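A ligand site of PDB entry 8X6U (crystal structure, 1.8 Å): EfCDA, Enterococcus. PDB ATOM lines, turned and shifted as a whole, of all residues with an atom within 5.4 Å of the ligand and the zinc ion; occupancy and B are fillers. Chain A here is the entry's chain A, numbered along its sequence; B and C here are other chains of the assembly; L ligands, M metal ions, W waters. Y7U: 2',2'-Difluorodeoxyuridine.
An oxygen (O5) of the ligand sits close to the backbone NH (N) of Cys 90 (2.6 Å).
O4 of the ligand sits at hydrogen-bond distance from OE2 of Glu 48 (2.5 Å).
N2 of the ligand sits at hydrogen-bond distance from OE1 of Glu 59, 2.9 Å away.
O4 of the ligand lies within hydrogen-bond range of ND2 of Asn 46 (2.8 Å).
The backbone carbonyl oxygen (O) of Ala 50 of chain B lies within hydrogen-bond range of an oxygen (O3) of the ligand (2.8 Å).
The backbone NH of Phe 52 of chain B lies within hydrogen-bond range of an oxygen (O3) of the ligand, 2.9 Å away.
The backbone NH (N) of Ala 58 sits at hydrogen-bond distance from an oxygen (O1) of the ligand, 3.0 Å away.
The side-chain sulfur (SG) of Cys 93 sits close to the side-chain carboxylate (OE1) of Glu 59 (3.7 Å).
NE of Arg 60 lies close to SG of Cys 93.
The side-chain sulfur (SG) of Cys 90 sits close to the side-chain hydroxyl (OG) of Ser 51 of chain B (3.3 Å).
The side-chain sulfur (SG) of Cys 90 sits close to the backbone NH (N) of Ala 92, at 3.5 Å.
N of Val 30 sits at hydrogen-bond distance from OD1 of Asn 46 (2.9 Å).
The side-chain amide nitrogen (ND2) of Asn 46 sits at hydrogen-bond distance from the backbone carbonyl oxygen (O) of Phe 28, at 2.9 Å.
The backbone NH (N) of Ser 51 of chain B sits at hydrogen-bond distance from the side-chain amide oxygen (OD1) of Asn 49 of chain B (2.9 Å).
The backbone NH (N) of Phe 28 is in hydrogen-bond range of the side-chain hydroxyl (OG) of Ser 26 (3.0 Å).
Val 23 touches the ligand (CG1 to O4, 3.8 Å).
OG of Ser 26 touches C8 of the ligand, at 3.9 Å.
Phe 28 touches the ligand.
Val 30 touches the ligand (CB to O1, 3.3 Å).
Thr 55 touches the ligand (CG2 to F1, 3.2 Å).
Asn 56 touches the ligand (O to F1, 3.8 Å).
CA of Pro 89 touches O5 of the ligand (3.5 Å).
Ser 51 of chain B touches the ligand (CA to O3, 3.4 Å).
Hydrophobic or aromatic side chains that line the ligand: Val 23, Phe 28, Val 30, Ala 58 and Phe 52 of chain B.
Within 4 Å of the ligand: Val 23, Ser 26, Phe 28, Val 30, Asn 46, Glu 48, Thr 55, Asn 56, Cys 57, Ala 58, Glu 59, Pro 89, Cys 90, Cys 93, Ala 50 of chain B, Ser 51 of chain B and Phe 52 of chain B.
Along chain A the residues within 4 Å of the ligand span positions 23 to 93.
The nearest printed residue that does not touch the ligand is Phe 129 of chain C (4.1 Å).
Of the 26 residues printed, 3 come within 4 Å of the zinc ion.
The nearest printed residue that does not touch the zinc ion is Ser 51 of chain B (4.1 Å).
The zinc ion is bound by SG of Cys 93, SG of Cys 90, SG of Cys 57 and O5 of the ligand.
The zinc ion has four donor atoms within binding distance.
Water W1 bridges OG of Ser 51 of chain B (2.7 Å) and N of Gly 53 of chain B (2.7 Å).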
ATOM      1  N   VAL A  23       0.834  -3.196  12.395  1.00  0.00           N
ATOM      2  CA  VAL A  23       1.327  -4.146  11.401  1.00  0.00           C
ATOM      3  C   VAL A  23       1.212  -3.568   9.996  1.00  0.00           C
ATOM      4  O   VAL A  23       0.615  -4.196   9.125  1.00  0.00           O
ATOM      5  CB  VAL A  23       0.597  -5.501  11.491  1.00  0.00           C
ATOM      6  CG1 VAL A  23       1.074  -6.271  12.761  1.00  0.00           C
ATOM      7  CG2 VAL A  23      -0.919  -5.324  11.526  1.00  0.00           C
ATOM      8  N   SER A  26       3.141  -6.536   7.399  1.00  0.00           N
ATOM      9  CA  SER A  26       2.521  -7.842   7.188  1.00  0.00           C
ATOM     10  C   SER A  26       1.010  -7.765   7.067  1.00  0.00           C
ATOM     11  O   SER A  26       0.406  -8.661   6.472  1.00  0.00           O
ATOM     12  CB  SER A  26       2.849  -8.780   8.343  1.00  0.00           C
ATOM     13  OG  SER A  26       2.105  -8.409   9.498  1.00  0.00           O
ATOM     14  N   PHE A  28      -0.884  -8.507   9.376  1.00  0.00           N
ATOM     15  CA  PHE A  28      -1.240  -9.735  10.078  1.00  0.00           C
ATOM     16  C   PHE A  28      -1.212  -9.430  11.579  1.00  0.00           C
ATOM     17  O   PHE A  28      -0.158  -9.550  12.229  1.00  0.00           O
ATOM     18  CB  PHE A  28      -0.263 -10.863   9.727  1.00  0.00           C
ATOM     19  CG  PHE A  28      -0.608 -12.195  10.313  1.00  0.00           C
ATOM     20  CD1 PHE A  28      -1.525 -13.021   9.703  1.00  0.00           C
ATOM     21  CD2 PHE A  28       0.015 -12.641  11.487  1.00  0.00           C
ATOM     22  CE1 PHE A  28      -1.837 -14.264  10.240  1.00  0.00           C
ATOM     23  CE2 PHE A  28      -0.291 -13.870  12.031  1.00  0.00           C
ATOM     24  CZ  PHE A  28      -1.229 -14.685  11.418  1.00  0.00           C
ATOM     25  N   VAL A  30      -1.793  -9.720  15.679  1.00  0.00           N
ATOM     26  CA  VAL A  30      -1.809 -10.734  16.721  1.00  0.00           C
ATOM     27  C   VAL A  30      -2.061 -10.011  18.034  1.00  0.00           C
ATOM     28  O   VAL A  30      -1.572  -8.906  18.242  1.00  0.00           O
ATOM     29  CB  VAL A  30      -0.494 -11.552  16.769  1.00  0.00           C
ATOM     30  CG1 VAL A  30      -0.579 -12.638  17.832  1.00  0.00           C
ATOM     31  CG2 VAL A  30      -0.217 -12.196  15.431  1.00  0.00           C
ATOM     32  N   ASN A  46       1.326  -7.007  18.384  1.00  0.00           N
ATOM     33  CA  ASN A  46       2.574  -7.012  17.626  1.00  0.00           C
ATOM     34  C   ASN A  46       2.854  -5.606  17.070  1.00  0.00           C
ATOM     35  O   ASN A  46       1.942  -4.822  16.819  1.00  0.00           O
ATOM     36  CB  ASN A  46       2.591  -8.099  16.531  1.00  0.00           C
ATOM     37  CG  ASN A  46       1.340  -8.132  15.644  1.00  0.00           C
ATOM     38  OD1 ASN A  46       0.263  -7.648  15.977  1.00  0.00           O
ATOM     39  ND2 ASN A  46       1.490  -8.820  14.517  1.00  0.00           N
ATOM     40  N   ILE A  47       4.146  -5.281  16.971  1.00  0.00           N
ATOM     41  CA  ILE A  47       4.615  -3.938  16.637  1.00  0.00           C
ATOM     42  C   ILE A  47       5.751  -4.092  15.642  1.00  0.00           C
ATOM     43  O   ILE A  47       6.858  -4.489  16.020  1.00  0.00           O
ATOM     44  CB  ILE A  47       5.082  -3.172  17.891  1.00  0.00           C
ATOM     45  CG1 ILE A  47       3.945  -3.050  18.921  1.00  0.00           C
ATOM     46  CG2 ILE A  47       5.628  -1.781  17.482  1.00  0.00           C
ATOM     47  CD1 ILE A  47       4.364  -2.401  20.264  1.00  0.00           C
ATOM     48  N   GLU A  48       5.496  -3.782  14.381  1.00  0.00           N
ATOM     49  CA  GLU A  48       6.488  -4.053  13.339  1.00  0.00           C
ATOM     50  C   GLU A  48       7.418  -2.876  13.152  1.00  0.00           C
ATOM     51  O   GLU A  48       7.238  -1.786  13.710  1.00  0.00           O
ATOM     52  CB  GLU A  48       5.782  -4.435  12.034  1.00  0.00           C
ATOM     53  CG  GLU A  48       4.905  -5.686  12.227  1.00  0.00           C
ATOM     54  CD  GLU A  48       4.271  -6.234  10.969  1.00  0.00           C
ATOM     55  OE1 GLU A  48       4.020  -5.459   9.999  1.00  0.00           O
ATOM     56  OE2 GLU A  48       3.927  -7.444  10.991  1.00  0.00           O
ATOM     57  N   THR A  55      10.811  -6.211  14.512  1.00  0.00           N
ATOM     58  CA  THR A  55       9.424  -6.432  14.897  1.00  0.00           C
ATOM     59  C   THR A  55       9.357  -7.137  16.239  1.00  0.00           C
ATOM     60  O   THR A  55      10.143  -8.053  16.524  1.00  0.00           O
ATOM     61  CB  THR A  55       8.722  -7.283  13.833  1.00  0.00           C
ATOM     62  OG1 THR A  55       8.650  -6.544  12.616  1.00  0.00           O
ATOM     63  CG2 THR A  55       7.314  -7.767  14.285  1.00  0.00           C
ATOM     64  N   ASN A  56       8.393  -6.726  17.058  1.00  0.00           N
ATOM     65  CA  ASN A  56       8.103  -7.392  18.332  1.00  0.00           C
ATOM     66  C   ASN A  56       6.715  -8.020  18.314  1.00  0.00           C
ATOM     67  O   ASN A  56       5.733  -7.358  17.968  1.00  0.00           O
ATOM     68  CB  ASN A  56       8.185  -6.409  19.492  1.00  0.00           C
ATOM     69  CG  ASN A  56       8.441  -7.106  20.787  1.00  0.00           C
ATOM     70  OD1 ASN A  56       9.391  -7.869  20.916  1.00  0.00           O
ATOM     71  ND2 ASN A  56       7.528  -6.926  21.740  1.00  0.00           N
ATOM     72  N   CYS A  57       6.636  -9.285  18.722  1.00  0.00           N
ATOM     73  CA  CYS A  57       5.379 -10.036  18.780  1.00  0.00           C
ATOM     74  C   CYS A  57       4.461  -9.565  19.899  1.00  0.00           C
ATOM     75  O   CYS A  57       4.890  -9.019  20.913  1.00  0.00           O
ATOM     76  CB  CYS A  57       5.663 -11.520  19.011  1.00  0.00           C
ATOM     77  SG  CYS A  57       6.530 -12.307  17.674  1.00  0.00           S
ATOM     78  N   ALA A  58       3.166  -9.882  19.731  1.00  0.00           N
ATOM     79  CA  ALA A  58       2.157  -9.519  20.730  1.00  0.00           C
ATOM     80  C   ALA A  58       2.453 -10.165  22.082  1.00  0.00           C
ATOM     81  O   ALA A  58       2.325  -9.521  23.129  1.00  0.00           O
ATOM     82  CB  ALA A  58       0.776  -9.918  20.247  1.00  0.00           C
ATOM     83  N   GLU A  59       2.852 -11.440  22.075  1.00  0.00           N
ATOM     84  CA  GLU A  59       3.130 -12.131  23.340  1.00  0.00           C
ATOM     85  C   GLU A  59       4.259 -11.425  24.103  1.00  0.00           C
ATOM     86  O   GLU A  59       4.141 -11.133  25.295  1.00  0.00           O
ATOM     87  CB  GLU A  59       3.492 -13.586  23.069  1.00  0.00           C
ATOM     88  CG  GLU A  59       2.414 -14.367  22.303  1.00  0.00           C
ATOM     89  CD  GLU A  59       2.575 -14.302  20.793  1.00  0.00           C
ATOM     90  OE1 GLU A  59       2.739 -13.199  20.257  1.00  0.00           O
ATOM     91  OE2 GLU A  59       2.563 -15.368  20.157  1.00  0.00           O
ATOM     92  N   ARG A  60       5.349 -11.120  23.396  1.00  0.00           N
ATOM     93  CA  ARG A  60       6.452 -10.446  24.042  1.00  0.00           C
ATOM     94  C   ARG A  60       6.098  -9.036  24.473  1.00  0.00           C
ATOM     95  O   ARG A  60       6.533  -8.592  25.545  1.00  0.00           O
ATOM     96  CB  ARG A  60       7.688 -10.454  23.128  1.00  0.00           C
ATOM     97  CG  ARG A  60       8.266 -11.880  23.052  1.00  0.00           C
ATOM     98  CD  ARG A  60       9.510 -11.941  22.192  1.00  0.00           C
ATOM     99  NE  ARG A  60       9.184 -11.981  20.766  1.00  0.00           N
ATOM    100  CZ  ARG A  60      10.038 -11.614  19.812  1.00  0.00           C
ATOM    101  NH1 ARG A  60      11.268 -11.204  20.105  1.00  0.00           N
ATOM    102  NH2 ARG A  60       9.656 -11.703  18.538  1.00  0.00           N
ATOM    103  N   SER A  88      -0.682 -19.791  16.546  1.00  0.00           N
ATOM    104  CA  SER A  88       0.447 -20.425  17.198  1.00  0.00           C
ATOM    105  C   SER A  88       1.499 -19.392  17.584  1.00  0.00           C
ATOM    106  O   SER A  88       1.960 -18.631  16.722  1.00  0.00           O
ATOM    107  CB  SER A  88       1.064 -21.462  16.260  1.00  0.00           C
ATOM    108  OG  SER A  88       2.348 -21.836  16.731  1.00  0.00           O
ATOM    109  N   PRO A  89       1.929 -19.355  18.854  1.00  0.00           N
ATOM    110  CA  PRO A  89       3.034 -18.478  19.230  1.00  0.00           C
ATOM    111  C   PRO A  89       4.332 -18.935  18.578  1.00  0.00           C
ATOM    112  O   PRO A  89       4.622 -20.139  18.522  1.00  0.00           O
ATOM    113  CB  PRO A  89       3.103 -18.604  20.753  1.00  0.00           C
ATOM    114  CG  PRO A  89       1.759 -19.184  21.166  1.00  0.00           C
ATOM    115  CD  PRO A  89       1.393 -20.085  20.021  1.00  0.00           C
ATOM    116  N   CYS A  90       5.110 -17.980  18.087  1.00  0.00           N
ATOM    117  CA  CYS A  90       6.407 -18.332  17.514  1.00  0.00           C
ATOM    118  C   CYS A  90       7.394 -18.748  18.592  1.00  0.00           C
ATOM    119  O   CYS A  90       7.192 -18.534  19.789  1.00  0.00           O
ATOM    120  CB  CYS A  90       6.955 -17.164  16.680  1.00  0.00           C
ATOM    121  SG  CYS A  90       7.897 -15.920  17.586  1.00  0.00           S
ATOM    122  N   GLY A  91       8.488 -19.381  18.145  1.00  0.00           N
ATOM    123  CA  GLY A  91       9.470 -19.916  19.071  1.00  0.00           C
ATOM    124  C   GLY A  91      10.110 -18.846  19.953  1.00  0.00           C
ATOM    125  O   GLY A  91      10.439 -19.103  21.108  1.00  0.00           O
ATOM    126  N   ALA A  92      10.330 -17.646  19.400  1.00  0.00           N
ATOM    127  CA  ALA A  92      10.939 -16.593  20.208  1.00  0.00           C
ATOM    128  C   ALA A  92      10.045 -16.250  21.390  1.00  0.00           C
ATOM    129  O   ALA A  92      10.528 -16.087  22.536  1.00  0.00           O
ATOM    130  CB  ALA A  92      11.203 -15.348  19.347  1.00  0.00           C
ATOM    131  N   CYS A  93       8.735 -16.145  21.148  1.00  0.00           N
ATOM    132  CA  CYS A  93       7.786 -15.864  22.216  1.00  0.00           C
ATOM    133  C   CYS A  93       7.763 -16.997  23.225  1.00  0.00           C
ATOM    134  O   CYS A  93       7.693 -16.762  24.436  1.00  0.00           O
ATOM    135  CB  CYS A  93       6.404 -15.653  21.641  1.00  0.00           C
ATOM    136  SG  CYS A  93       6.322 -14.076  20.783  1.00  0.00           S
ATOM    137  N   ASN B  49      11.770 -14.636   7.972  1.00  0.00           N
ATOM    138  CA  ASN B  49      11.102 -15.677   8.736  1.00  0.00           C
ATOM    139  C   ASN B  49       9.620 -15.351   8.792  1.00  0.00           C
ATOM    140  O   ASN B  49       9.251 -14.174   8.858  1.00  0.00           O
ATOM    141  CB  ASN B  49      11.663 -15.779  10.180  1.00  0.00           C
ATOM    142  CG  ASN B  49      11.206 -17.038  10.900  1.00  0.00           C
ATOM    143  OD1 ASN B  49      10.141 -17.052  11.537  1.00  0.00           O
ATOM    144  ND2 ASN B  49      11.998 -18.085  10.795  1.00  0.00           N
ATOM    145  N   ALA B  50       8.782 -16.388   8.786  1.00  0.00           N
ATOM    146  CA  ALA B  50       7.340 -16.178   8.898  1.00  0.00           C
ATOM    147  C   ALA B  50       6.987 -15.333  10.113  1.00  0.00           C
ATOM    148  O   ALA B  50       6.020 -14.575  10.087  1.00  0.00           O
ATOM    149  CB  ALA B  50       6.617 -17.528   8.985  1.00  0.00           C
ATOM    150  N   SER B  51       7.742 -15.480  11.207  1.00  0.00           N
ATOM    151  CA  SER B  51       7.689 -14.537  12.315  1.00  0.00           C
ATOM    152  C   SER B  51       8.690 -13.435  11.988  1.00  0.00           C
ATOM    153  O   SER B  51       9.914 -13.656  12.044  1.00  0.00           O
ATOM    154  CB  SER B  51       8.022 -15.238  13.634  1.00  0.00           C
ATOM    155  OG  SER B  51       7.894 -14.314  14.717  1.00  0.00           O
ATOM    156  N   PHE B  52       8.189 -12.250  11.600  1.00  0.00           N
ATOM    157  CA  PHE B  52       9.040 -11.248  10.961  1.00  0.00           C
ATOM    158  C   PHE B  52      10.245 -10.892  11.813  1.00  0.00           C
ATOM    159  O   PHE B  52      11.313 -10.619  11.277  1.00  0.00           O
ATOM    160  CB  PHE B  52       8.242  -9.987  10.638  1.00  0.00           C
ATOM    161  CG  PHE B  52       7.443 -10.060   9.349  1.00  0.00           C
ATOM    162  CD1 PHE B  52       7.202 -11.267   8.700  1.00  0.00           C
ATOM    163  CD2 PHE B  52       6.929  -8.888   8.785  1.00  0.00           C
ATOM    164  CE1 PHE B  52       6.464 -11.309   7.514  1.00  0.00           C
ATOM    165  CE2 PHE B  52       6.193  -8.917   7.597  1.00  0.00           C
ATOM    166  CZ  PHE B  52       5.959 -10.122   6.967  1.00  0.00           C
ATOM    167  N   GLY B  53      10.065 -10.854  13.141  1.00  0.00           N
ATOM    168  CA  GLY B  53      11.141 -10.441  14.028  1.00  0.00           C
ATOM    169  C   GLY B  53      12.324 -11.393  14.091  1.00  0.00           C
ATOM    170  O   GLY B  53      13.321 -11.061  14.745  1.00  0.00           O
ATOM    171  N   PHE C 129       4.191 -22.311  14.302  1.00  0.00           N
ATOM    172  CA  PHE C 129       3.756 -21.187  13.476  1.00  0.00           C
ATOM    173  C   PHE C 129       4.443 -21.249  12.119  1.00  0.00           C
ATOM    174  O   PHE C 129       5.661 -21.463  12.049  1.00  0.00           O
ATOM    175  CB  PHE C 129       4.100 -19.877  14.175  1.00  0.00           C
ATOM    176  CG  PHE C 129       3.677 -18.652  13.424  1.00  0.00           C
ATOM    177  CD1 PHE C 129       2.373 -18.200  13.469  1.00  0.00           C
ATOM    178  CD2 PHE C 129       4.607 -17.957  12.646  1.00  0.00           C
ATOM    179  CE1 PHE C 129       1.984 -17.069  12.764  1.00  0.00           C
ATOM    180  CE2 PHE C 129       4.228 -16.843  11.939  1.00  0.00           C
ATOM    181  CZ  PHE C 129       2.930 -16.377  11.991  1.00  0.00           C
ATOM    182  N   LEU C 134      -0.309 -15.824   6.262  1.00  0.00           N
ATOM    183  CA  LEU C 134       0.163 -14.467   5.990  1.00  0.00           C
ATOM    184  C   LEU C 134      -0.388 -13.974   4.669  1.00  0.00           C
ATOM    185  O   LEU C 134      -0.694 -14.773   3.774  1.00  0.00           O
ATOM    186  CB  LEU C 134       1.680 -14.432   5.974  1.00  0.00           C
ATOM    187  CG  LEU C 134       2.365 -14.837   7.272  1.00  0.00           C
ATOM    188  CD1 LEU C 134       3.868 -14.748   7.033  1.00  0.00           C
ATOM    189  CD2 LEU C 134       1.912 -13.952   8.436  1.00  0.00           C
ATOM    190  OXT LEU C 134      -0.552 -12.767   4.474  1.00  0.00           O
HETATM  191  N1  Y7U L   1       3.571 -12.565  15.357  1.00  0.00           N
HETATM  192  C2  Y7U L   1       4.134 -13.732  14.907  1.00  0.00           C
HETATM  193  O3  Y7U L   1       5.315 -12.221  11.502  1.00  0.00           O
HETATM  194  C4  Y7U L   1       4.143 -14.649  17.122  1.00  0.00           C
HETATM  195  C5  Y7U L   1       3.381 -11.417  14.448  1.00  0.00           C
HETATM  196  C6  Y7U L   1       4.708 -10.688  14.214  1.00  0.00           C
HETATM  197  C7  Y7U L   1       4.476  -9.970  12.888  1.00  0.00           C
HETATM  198  C9  Y7U L   1       4.126 -11.619  11.024  1.00  0.00           C
HETATM  199  C1  Y7U L   1       4.423 -14.766  15.718  1.00  0.00           C
HETATM  200  C3  Y7U L   1       3.285 -12.369  16.694  1.00  0.00           C
HETATM  201  C8  Y7U L   1       3.473 -10.881  12.176  1.00  0.00           C
HETATM  202  F1  Y7U L   1       5.131  -9.898  15.248  1.00  0.00           F
HETATM  203  F2  Y7U L   1       5.706 -11.611  14.067  1.00  0.00           F
HETATM  204  N2  Y7U L   1       3.575 -13.447  17.496  1.00  0.00           N
HETATM  205  O1  Y7U L   1       2.789 -11.351  17.149  1.00  0.00           O
HETATM  206  O2  Y7U L   1       3.033 -11.863  13.151  1.00  0.00           O
HETATM  207  O4  Y7U L   1       3.954  -8.683  13.144  1.00  0.00           O
HETATM  208  O5  Y7U L   1       4.351 -15.493  17.995  1.00  0.00           O
HETATM  209 ZN    ZN M   1       6.390 -14.452  18.533  1.00  0.00          ZN
HETATM  210  O   HOH W   1       8.474 -11.697  15.204  1.00  0.00           O
